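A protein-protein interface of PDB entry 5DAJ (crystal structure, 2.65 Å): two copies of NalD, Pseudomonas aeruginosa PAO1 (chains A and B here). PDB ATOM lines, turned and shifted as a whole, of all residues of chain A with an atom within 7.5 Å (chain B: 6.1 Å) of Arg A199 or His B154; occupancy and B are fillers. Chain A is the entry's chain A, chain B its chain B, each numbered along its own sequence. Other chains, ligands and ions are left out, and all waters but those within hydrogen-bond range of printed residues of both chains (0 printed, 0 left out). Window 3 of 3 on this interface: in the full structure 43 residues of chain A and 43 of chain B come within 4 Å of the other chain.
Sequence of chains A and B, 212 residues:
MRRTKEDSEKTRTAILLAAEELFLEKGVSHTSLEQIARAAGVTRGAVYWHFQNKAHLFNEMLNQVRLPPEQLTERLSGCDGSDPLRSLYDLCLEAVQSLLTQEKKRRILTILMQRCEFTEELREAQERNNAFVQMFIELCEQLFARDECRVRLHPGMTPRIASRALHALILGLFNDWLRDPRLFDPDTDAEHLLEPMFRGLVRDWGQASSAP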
ATOM      1  N   ARG A 152       6.233   0.238  -2.831  1.00  0.00           N
ATOM      2  CA  ARG A 152       7.309  -0.029  -1.872  1.00  0.00           C
ATOM      3  C   ARG A 152       7.217   0.751  -0.564  1.00  0.00           C
ATOM      4  O   ARG A 152       8.002   0.510   0.353  1.00  0.00           O
ATOM      5  CB  ARG A 152       8.663   0.256  -2.516  1.00  0.00           C
ATOM      6  CG  ARG A 152       8.883  -0.445  -3.850  1.00  0.00           C
ATOM      7  CD  ARG A 152      10.300  -0.248  -4.355  1.00  0.00           C
ATOM      8  NE  ARG A 152      11.287  -0.661  -3.357  1.00  0.00           N
ATOM      9  CZ  ARG A 152      12.585  -0.366  -3.390  1.00  0.00           C
ATOM     10  NH1 ARG A 152      13.106   0.344  -4.396  1.00  0.00           N
ATOM     11  NH2 ARG A 152      13.375  -0.792  -2.402  1.00  0.00           N
ATOM     12  N   HIS A 154       5.628   1.853   3.073  1.00  0.00           N
ATOM     13  CA  HIS A 154       4.909   1.135   4.135  1.00  0.00           C
ATOM     14  C   HIS A 154       3.431   1.533   4.142  1.00  0.00           C
ATOM     15  O   HIS A 154       3.086   2.614   3.658  1.00  0.00           O
ATOM     16  CB  HIS A 154       5.498   1.369   5.540  1.00  0.00           C
ATOM     17  CG  HIS A 154       6.759   0.620   5.815  1.00  0.00           C
ATOM     18  ND1 HIS A 154       7.975   0.993   5.292  1.00  0.00           N
ATOM     19  CD2 HIS A 154       6.997  -0.471   6.582  1.00  0.00           C
ATOM     20  CE1 HIS A 154       8.910   0.157   5.710  1.00  0.00           C
ATOM     21  NE2 HIS A 154       8.345  -0.742   6.495  1.00  0.00           N
ATOM     22  N   LEU A 194      20.810   9.635   7.320  1.00  0.00           N
ATOM     23  CA  LEU A 194      19.735   9.444   6.342  1.00  0.00           C
ATOM     24  C   LEU A 194      19.131   8.037   6.368  1.00  0.00           C
ATOM     25  O   LEU A 194      17.942   7.865   6.081  1.00  0.00           O
ATOM     26  CB  LEU A 194      20.239   9.752   4.927  1.00  0.00           C
ATOM     27  CG  LEU A 194      20.721  11.180   4.693  1.00  0.00           C
ATOM     28  CD1 LEU A 194      21.368  11.289   3.329  1.00  0.00           C
ATOM     29  CD2 LEU A 194      19.584  12.183   4.812  1.00  0.00           C
ATOM     30  N   GLU A 195      19.953   7.051   6.719  1.00  0.00           N
ATOM     31  CA  GLU A 195      19.539   5.642   6.744  1.00  0.00           C
ATOM     32  C   GLU A 195      18.142   5.398   7.340  1.00  0.00           C
ATOM     33  O   GLU A 195      17.275   4.845   6.649  1.00  0.00           O
ATOM     34  CB  GLU A 195      20.597   4.772   7.452  1.00  0.00           C
ATOM     35  CG  GLU A 195      20.337   3.263   7.480  1.00  0.00           C
ATOM     36  CD  GLU A 195      20.284   2.606   6.105  1.00  0.00           C
ATOM     37  OE1 GLU A 195      20.594   3.262   5.076  1.00  0.00           O
ATOM     38  OE2 GLU A 195      19.934   1.404   6.060  1.00  0.00           O
ATOM     39  N   PRO A 196      17.906   5.821   8.599  1.00  0.00           N
ATOM     40  CA  PRO A 196      16.622   5.483   9.226  1.00  0.00           C
ATOM     41  C   PRO A 196      15.409   6.051   8.497  1.00  0.00           C
ATOM     42  O   PRO A 196      14.390   5.378   8.396  1.00  0.00           O
ATOM     43  CB  PRO A 196      16.741   6.092  10.625  1.00  0.00           C
ATOM     44  CG  PRO A 196      17.771   7.155  10.499  1.00  0.00           C
ATOM     45  CD  PRO A 196      18.745   6.636   9.494  1.00  0.00           C
ATOM     46  N   MET A 197      15.527   7.266   7.972  1.00  0.00           N
ATOM     47  CA  MET A 197      14.419   7.881   7.229  1.00  0.00           C
ATOM     48  C   MET A 197      14.044   7.004   6.066  1.00  0.00           C
ATOM     49  O   MET A 197      12.869   6.673   5.885  1.00  0.00           O
ATOM     50  CB  MET A 197      14.755   9.290   6.750  1.00  0.00           C
ATOM     51  CG  MET A 197      13.674   9.939   5.877  1.00  0.00           C
ATOM     52  SD  MET A 197      11.932  10.036   6.812  1.00  0.00           S
ATOM     53  CE  MET A 197      12.324  11.576   7.978  1.00  0.00           C
ATOM     54  N   PHE A 198      15.035   6.615   5.271  1.00  0.00           N
ATOM     55  CA  PHE A 198      14.778   5.760   4.099  1.00  0.00           C
ATOM     56  C   PHE A 198      14.330   4.348   4.460  1.00  0.00           C
ATOM     57  O   PHE A 198      13.459   3.788   3.788  1.00  0.00           O
ATOM     58  CB  PHE A 198      15.983   5.709   3.175  1.00  0.00           C
ATOM     59  CG  PHE A 198      16.109   6.922   2.315  1.00  0.00           C
ATOM     60  CD1 PHE A 198      16.754   8.056   2.789  1.00  0.00           C
ATOM     61  CD2 PHE A 198      15.541   6.953   1.049  1.00  0.00           C
ATOM     62  CE1 PHE A 198      16.861   9.188   2.002  1.00  0.00           C
ATOM     63  CE2 PHE A 198      15.653   8.080   0.259  1.00  0.00           C
ATOM     64  CZ  PHE A 198      16.312   9.198   0.735  1.00  0.00           C
ATOM     65  N   ARG A 199      14.861   3.812   5.554  1.00  0.00           N
ATOM     66  CA  ARG A 199      14.454   2.495   6.022  1.00  0.00           C
ATOM     67  C   ARG A 199      13.004   2.568   6.512  1.00  0.00           C
ATOM     68  O   ARG A 199      12.229   1.630   6.327  1.00  0.00           O
ATOM     69  CB  ARG A 199      15.372   2.015   7.147  1.00  0.00           C
ATOM     70  CG  ARG A 199      15.226   0.539   7.480  1.00  0.00           C
ATOM     71  CD  ARG A 199      15.902   0.201   8.798  1.00  0.00           C
ATOM     72  NE  ARG A 199      17.356   0.300   8.708  1.00  0.00           N
ATOM     73  CZ  ARG A 199      18.178  -0.744   8.721  1.00  0.00           C
ATOM     74  NH1 ARG A 199      17.690  -1.974   8.821  1.00  0.00           N
ATOM     75  NH2 ARG A 199      19.489  -0.560   8.634  1.00  0.00           N
ATOM     76  N   GLY A 200      12.648   3.691   7.134  1.00  0.00           N
ATOM     77  CA  GLY A 200      11.290   3.913   7.646  1.00  0.00           C
ATOM     78  C   GLY A 200      10.226   4.158   6.592  1.00  0.00           C
ATOM     79  O   GLY A 200       9.046   3.885   6.811  1.00  0.00           O
ATOM     80  N   LEU A 201      10.635   4.710   5.456  1.00  0.00           N
ATOM     81  CA  LEU A 201       9.717   4.978   4.339  1.00  0.00           C
ATOM     82  C   LEU A 201       9.506   3.762   3.445  1.00  0.00           C
ATOM     83  O   LEU A 201       8.384   3.508   3.007  1.00  0.00           O
ATOM     84  CB  LEU A 201      10.228   6.137   3.479  1.00  0.00           C
ATOM     85  CG  LEU A 201      10.225   7.532   4.111  1.00  0.00           C
ATOM     86  CD1 LEU A 201      10.994   8.505   3.228  1.00  0.00           C
ATOM     87  CD2 LEU A 201       8.816   8.042   4.341  1.00  0.00           C
ATOM     88  N   VAL A 202      10.584   3.031   3.179  1.00  0.00           N
ATOM     89  CA  VAL A 202      10.608   1.991   2.131  1.00  0.00           C
ATOM     90  C   VAL A 202      10.756   0.570   2.701  1.00  0.00           C
ATOM     91  O   VAL A 202      11.586   0.319   3.572  1.00  0.00           O
ATOM     92  CB  VAL A 202      11.730   2.272   1.110  1.00  0.00           C
ATOM     93  CG1 VAL A 202      11.710   1.258  -0.027  1.00  0.00           C
ATOM     94  CG2 VAL A 202      11.580   3.672   0.534  1.00  0.00           C
ATOM     95  N   ARG A 203       9.962  -0.347   2.151  1.00  0.00           N
ATOM     96  CA  ARG A 203       9.819  -1.723   2.678  1.00  0.00           C
ATOM     97  C   ARG A 203      11.112  -2.516   2.763  1.00  0.00           C
ATOM     98  O   ARG A 203      11.432  -3.066   3.817  1.00  0.00           O
ATOM     99  CB  ARG A 203       8.796  -2.543   1.870  1.00  0.00           C
ATOM    100  CG  ARG A 203       7.442  -2.664   2.544  1.00  0.00           C
ATOM    101  CD  ARG A 203       6.462  -3.400   1.653  1.00  0.00           C
ATOM    102  NE  ARG A 203       5.064  -3.080   1.807  1.00  0.00           N
ATOM    103  CZ  ARG A 203       4.265  -3.339   2.841  1.00  0.00           C
ATOM    104  NH1 ARG A 203       4.707  -3.885   3.973  1.00  0.00           N
ATOM    105  NH2 ARG A 203       2.981  -2.997   2.737  1.00  0.00           N
ATOM    106  N   ASP A 204      11.842  -2.581   1.654  1.00  0.00           N
ATOM    107  CA  ASP A 204      13.000  -3.475   1.571  1.00  0.00           C
ATOM    108  C   ASP A 204      14.272  -2.834   2.106  1.00  0.00           C
ATOM    109  O   ASP A 204      14.894  -3.364   3.017  1.00  0.00           O
ATOM    110  CB  ASP A 204      13.192  -4.000   0.139  1.00  0.00           C
ATOM    111  CG  ASP A 204      12.383  -5.278  -0.140  1.00  0.00           C
ATOM    112  OD1 ASP A 204      11.764  -5.845   0.795  1.00  0.00           O
ATOM    113  OD2 ASP A 204      12.374  -5.724  -1.308  1.00  0.00           O
ATOM    114  N   TRP A 205      14.643  -1.694   1.540  1.00  0.00           N
ATOM    115  CA  TRP A 205      15.891  -0.980   1.876  1.00  0.00           C
ATOM    116  C   TRP A 205      16.972  -1.855   2.508  1.00  0.00           C
ATOM    117  O   TRP A 205      18.077  -1.952   1.985  1.00  0.00           O
ATOM    118  CB  TRP A 205      15.625   0.226   2.789  1.00  0.00           C
ATOM    119  CG  TRP A 205      16.614   1.312   2.555  1.00  0.00           C
ATOM    120  CD1 TRP A 205      17.652   1.666   3.366  1.00  0.00           C
ATOM    121  CD2 TRP A 205      16.702   2.149   1.402  1.00  0.00           C
ATOM    122  NE1 TRP A 205      18.372   2.693   2.795  1.00  0.00           N
ATOM    123  CE2 TRP A 205      17.809   3.008   1.589  1.00  0.00           C
ATOM    124  CE3 TRP A 205      15.950   2.264   0.231  1.00  0.00           C
ATOM    125  CZ2 TRP A 205      18.176   3.977   0.652  1.00  0.00           C
ATOM    126  CZ3 TRP A 205      16.319   3.223  -0.702  1.00  0.00           C
ATOM    127  CH2 TRP A 205      17.419   4.067  -0.486  1.00  0.00           C
ATOM    128  N   ARG B 150      19.140   0.679  23.695  1.00  0.00           N
ATOM    129  CA  ARG B 150      20.237   0.398  22.741  1.00  0.00           C
ATOM    130  C   ARG B 150      20.085  -0.938  22.010  1.00  0.00           C
ATOM    131  O   ARG B 150      20.298  -1.020  20.799  1.00  0.00           O
ATOM    132  CB  ARG B 150      21.589   0.432  23.469  1.00  0.00           C
ATOM    133  CG  ARG B 150      22.808   0.190  22.601  1.00  0.00           C
ATOM    134  CD  ARG B 150      24.105  -0.034  23.397  1.00  0.00           C
ATOM    135  NE  ARG B 150      24.931   1.169  23.342  1.00  0.00           N
ATOM    136  CZ  ARG B 150      25.637   1.559  22.280  1.00  0.00           C
ATOM    137  NH1 ARG B 150      25.638   0.846  21.156  1.00  0.00           N
ATOM    138  NH2 ARG B 150      26.342   2.674  22.344  1.00  0.00           N
ATOM    139  N   VAL B 151      19.704  -1.969  22.760  1.00  0.00           N
ATOM    140  CA  VAL B 151      19.435  -3.312  22.212  1.00  0.00           C
ATOM    141  C   VAL B 151      18.378  -3.304  21.088  1.00  0.00           C
ATOM    142  O   VAL B 151      18.387  -4.168  20.205  1.00  0.00           O
ATOM    143  CB  VAL B 151      19.017  -4.284  23.347  1.00  0.00           C
ATOM    144  CG1 VAL B 151      18.404  -5.571  22.811  1.00  0.00           C
ATOM    145  CG2 VAL B 151      20.222  -4.626  24.209  1.00  0.00           C
ATOM    146  N   ARG B 152      17.480  -2.321  21.135  1.00  0.00           N
ATOM    147  CA  ARG B 152      16.387  -2.180  20.172  1.00  0.00           C
ATOM    148  C   ARG B 152      16.729  -1.372  18.914  1.00  0.00           C
ATOM    149  O   ARG B 152      15.922  -1.324  17.987  1.00  0.00           O
ATOM    150  CB  ARG B 152      15.178  -1.538  20.843  1.00  0.00           C
ATOM    151  CG  ARG B 152      14.737  -2.221  22.132  1.00  0.00           C
ATOM    152  CD  ARG B 152      13.444  -1.628  22.655  1.00  0.00           C
ATOM    153  NE  ARG B 152      12.392  -1.649  21.635  1.00  0.00           N
ATOM    154  CZ  ARG B 152      11.243  -0.975  21.697  1.00  0.00           C
ATOM    155  NH1 ARG B 152      10.951  -0.205  22.751  1.00  0.00           N
ATOM    156  NH2 ARG B 152      10.373  -1.077  20.689  1.00  0.00           N
ATOM    157  N   LEU B 153      17.897  -0.731  18.880  1.00  0.00           N
ATOM    158  CA  LEU B 153      18.340  -0.015  17.681  1.00  0.00           C
ATOM    159  C   LEU B 153      18.766  -1.001  16.602  1.00  0.00           C
ATOM    160  O   LEU B 153      19.203  -2.107  16.916  1.00  0.00           O
ATOM    161  CB  LEU B 153      19.502   0.927  17.992  1.00  0.00           C
ATOM    162  CG  LEU B 153      19.242   2.076  18.968  1.00  0.00           C
ATOM    163  CD1 LEU B 153      20.526   2.865  19.184  1.00  0.00           C
ATOM    164  CD2 LEU B 153      18.139   3.000  18.482  1.00  0.00           C
ATOM    165  N   HIS B 154      18.634  -0.604  15.336  1.00  0.00           N
ATOM    166  CA  HIS B 154      19.106  -1.447  14.226  1.00  0.00           C
ATOM    167  C   HIS B 154      20.634  -1.520  14.230  1.00  0.00           C
ATOM    168  O   HIS B 154      21.288  -0.628  14.783  1.00  0.00           O
ATOM    169  CB  HIS B 154      18.633  -0.963  12.845  1.00  0.00           C
ATOM    170  CG  HIS B 154      17.203  -1.275  12.537  1.00  0.00           C
ATOM    171  ND1 HIS B 154      16.154  -0.575  13.087  1.00  0.00           N
ATOM    172  CD2 HIS B 154      16.651  -2.195  11.711  1.00  0.00           C
ATOM    173  CE1 HIS B 154      15.015  -1.061  12.630  1.00  0.00           C
ATOM    174  NE2 HIS B 154      15.288  -2.044  11.793  1.00  0.00           N
ATOM    175  N   PRO B 155      21.207  -2.584  13.627  1.00  0.00           N
ATOM    176  CA  PRO B 155      22.656  -2.725  13.482  1.00  0.00           C
ATOM    177  C   PRO B 155      23.289  -1.472  12.879  1.00  0.00           C
ATOM    178  O   PRO B 155      22.847  -1.015  11.830  1.00  0.00           O
ATOM    179  CB  PRO B 155      22.791  -3.882  12.489  1.00  0.00           C
ATOM    180  CG  PRO B 155      21.609  -4.734  12.768  1.00  0.00           C
ATOM    181  CD  PRO B 155      20.504  -3.798  13.170  1.00  0.00           C
ATOM    182  N   GLY B 156      24.279  -0.903  13.555  1.00  0.00           N
ATOM    183  CA  GLY B 156      24.988   0.282  13.044  1.00  0.00           C
ATOM    184  C   GLY B 156      24.336   1.630  13.323  1.00  0.00           C
ATOM    185  O   GLY B 156      24.879   2.668  12.938  1.00  0.00           O
ATOM    186  N   MET B 157      23.168   1.620  13.966  1.00  0.00           N
ATOM    187  CA  MET B 157      22.597   2.827  14.568  1.00  0.00           C
ATOM    188  C   MET B 157      23.180   2.987  15.946  1.00  0.00           C
ATOM    189  O   MET B 157      22.913   2.180  16.835  1.00  0.00           O
ATOM    190  CB  MET B 157      21.069   2.773  14.684  1.00  0.00           C
ATOM    191  CG  MET B 157      20.373   3.095  13.367  1.00  0.00           C
ATOM    192  SD  MET B 157      20.924   4.882  12.731  1.00  0.00           S
ATOM    193  CE  MET B 157      20.988   5.794  14.472  1.00  0.00           C
ATOM    194  N   THR B 158      23.972   4.038  16.128  1.00  0.00           N
ATOM    195  CA  THR B 158      24.494   4.405  17.440  1.00  0.00           C
ATOM    196  C   THR B 158      23.603   5.464  18.094  1.00  0.00           C
ATOM    197  O   THR B 158      22.885   6.193  17.395  1.00  0.00           O
ATOM    198  CB  THR B 158      25.925   4.966  17.347  1.00  0.00           C
ATOM    199  OG1 THR B 158      25.930   6.169  16.567  1.00  0.00           O
ATOM    200  CG2 THR B 158      26.850   3.941  16.710  1.00  0.00           C
ATOM    201  N   PRO B 196       8.227   7.256  10.145  1.00  0.00           N
ATOM    202  CA  PRO B 196       9.360   6.587   9.496  1.00  0.00           C
ATOM    203  C   PRO B 196      10.676   6.707  10.256  1.00  0.00           C
ATOM    204  O   PRO B 196      11.441   5.746  10.301  1.00  0.00           O
ATOM    205  CB  PRO B 196       9.456   7.284   8.131  1.00  0.00           C
ATOM    206  CG  PRO B 196       8.799   8.595   8.328  1.00  0.00           C
ATOM    207  CD  PRO B 196       7.698   8.340   9.305  1.00  0.00           C
ATOM    208  N   ARG B 199      10.433   4.233  13.078  1.00  0.00           N
ATOM    209  CA  ARG B 199      10.454   2.890  12.480  1.00  0.00           C
ATOM    210  C   ARG B 199      11.852   2.532  11.966  1.00  0.00           C
ATOM    211  O   ARG B 199      12.266   1.382  12.041  1.00  0.00           O
ATOM    212  CB  ARG B 199       9.436   2.776  11.340  1.00  0.00           C
ATOM    213  CG  ARG B 199       9.287   1.359  10.801  1.00  0.00           C
ATOM    214  CD  ARG B 199       7.954   1.085  10.115  1.00  0.00           C
ATOM    215  NE  ARG B 199       7.290   2.304   9.703  1.00  0.00           N
ATOM    216  N   GLY B 200      12.560   3.526  11.442  1.00  0.00           N
ATOM    217  CA  GLY B 200      13.925   3.351  10.937  1.00  0.00           C
ATOM    218  C   GLY B 200      15.004   3.202  11.998  1.00  0.00           C
ATOM    219  O   GLY B 200      16.040   2.591  11.755  1.00  0.00           O
ATOM    220  N   LEU B 201      14.772   3.784  13.169  1.00  0.00           N
ATOM    221  CA  LEU B 201      15.711   3.689  14.292  1.00  0.00           C
ATOM    222  C   LEU B 201      15.527   2.414  15.110  1.00  0.00           C
ATOM    223  O   LEU B 201      16.510   1.801  15.525  1.00  0.00           O
ATOM    224  CB  LEU B 201      15.566   4.893  15.226  1.00  0.00           C
ATOM    225  CG  LEU B 201      15.999   6.260  14.687  1.00  0.00           C
ATOM    226  CD1 LEU B 201      15.553   7.363  15.635  1.00  0.00           C
ATOM    227  CD2 LEU B 201      17.503   6.323  14.479  1.00  0.00           C
ATOM    228  N   VAL B 202      14.271   2.032  15.339  1.00  0.00           N
ATOM    229  CA  VAL B 202      13.915   0.987  16.322  1.00  0.00           C
ATOM    230  C   VAL B 202      13.343  -0.283  15.673  1.00  0.00           C
ATOM    231  O   VAL B 202      12.490  -0.214  14.787  1.00  0.00           O
ATOM    232  CB  VAL B 202      12.920   1.533  17.362  1.00  0.00           C
ATOM    233  CG1 VAL B 202      12.617   0.494  18.435  1.00  0.00           C
ATOM    234  CG2 VAL B 202      13.482   2.783  18.022  1.00  0.00           C
ATOM    235  N   ARG B 203      13.862  -1.411  16.113  1.00  0.00           N
ATOM    236  CA  ARG B 203      13.535  -2.728  15.602  1.00  0.00           C
ATOM    237  C   ARG B 203      12.097  -3.148  15.463  1.00  0.00           C
ATOM    238  O   ARG B 203      11.682  -3.609  14.416  1.00  0.00           O
ATOM    239  CB  ARG B 203      14.181  -3.759  16.506  1.00  0.00           C
ATOM    240  CG  ARG B 203      15.525  -4.291  16.052  1.00  0.00           C
ATOM    241  CD  ARG B 203      16.140  -5.121  17.163  1.00  0.00           C
ATOM    242  NE  ARG B 203      17.551  -5.394  16.943  1.00  0.00           N
ATOM    243  CZ  ARG B 203      18.069  -5.759  15.776  1.00  0.00           C
ATOM    244  NH1 ARG B 203      19.367  -5.990  15.667  1.00  0.00           N
ATOM    245  NH2 ARG B 203      17.289  -5.884  14.713  1.00  0.00           N
ATOM    246  N   ASP B 204      11.342  -3.017  16.532  1.00  0.00           N
ATOM    247  CA  ASP B 204       9.960  -3.511  16.569  1.00  0.00           C
ATOM    248  C   ASP B 204       8.950  -2.475  16.082  1.00  0.00           C
ATOM    249  O   ASP B 204       8.208  -2.734  15.141  1.00  0.00           O
ATOM    250  CB  ASP B 204       9.600  -4.037  17.965  1.00  0.00           C
ATOM    251  CG  ASP B 204       9.978  -5.515  18.160  1.00  0.00           C
ATOM    252  OD1 ASP B 204      10.405  -6.186  17.187  1.00  0.00           O
ATOM    253  OD2 ASP B 204       9.837  -6.010  19.298  1.00  0.00           O
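The backbone NH of His B154 sits at hydrogen-bond distance from the backbone carbonyl oxygen of Leu B201, 3.2 Å away. The backbone carbonyl oxygen of Gly B200 is in hydrogen-bond range of a ring nitrogen (ND1) of His B154 (3.4 Å). OE2 of Glu A195 is in salt-bridge range of NH2 of Arg A199 (3.3 Å). The backbone carbonyl oxygen (O) of Gly A200 lies within hydrogen-bond range of a ring nitrogen (ND1) of His A154 (3.4 Å). N of His A154 sits at hydrogen-bond distance from O of Leu A201, at 3.2 Å.
Among the printed residues, merely in contact across the chains: Arg A199 with His B154, Gly A200 with Pro B196, Pro A196 with Gly B200, Pro A196 with Pro B196, Gly A200 with Arg B199, Met A197 with Pro B196, Arg A199 with Gly B200, Leu A201 with Pro B196, Pro A196 with Leu B201 and His A154 with Arg B199.
Printed residues of chain B within 4 Å of His A154: Arg B199 (3.98 Å). Of the printed residues of chain B, Pro A196 touches Pro B196 (3.5 Å), Gly B200 (3.3 Å) and Leu B201 (3.9 Å). Arg A199 touches just these residues of chain B: His B154 and Gly B200. Printed residues of chain B within 4 Å of Gly A200: Pro B196 and Arg B199. Of the printed residues of chain A, Pro B196 touches Pro A196 (3.5 Å), Met A197 (3.8 Å), Gly A200 (3.2 Å) and Leu A201 (3.9 Å).
Of the 16 printed residues of chain B, 5 touch a printed residue of chain A. Printed residues of chain A that touch a printed residue of chain B: His A154, Pro A196, Met A197, Arg A199, Gly A200 and Leu A201. Hydrophobic or aromatic side chains of chain A that line the printed part of chain B: His A154, Pro A196, Met A197 and Leu A201.
His A154 touches Arg B199, and with the chains exchanged Arg A199 touches His B154. Pro B196 touches its own counterpart, Pro A196. Pro A196 touches Leu B201, and with the chains exchanged Leu A201 touches Pro B196. Arg A199 touches Gly B200, and with the chains exchanged Gly A200 touches Arg B199. 9 positions are printed for both chains.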
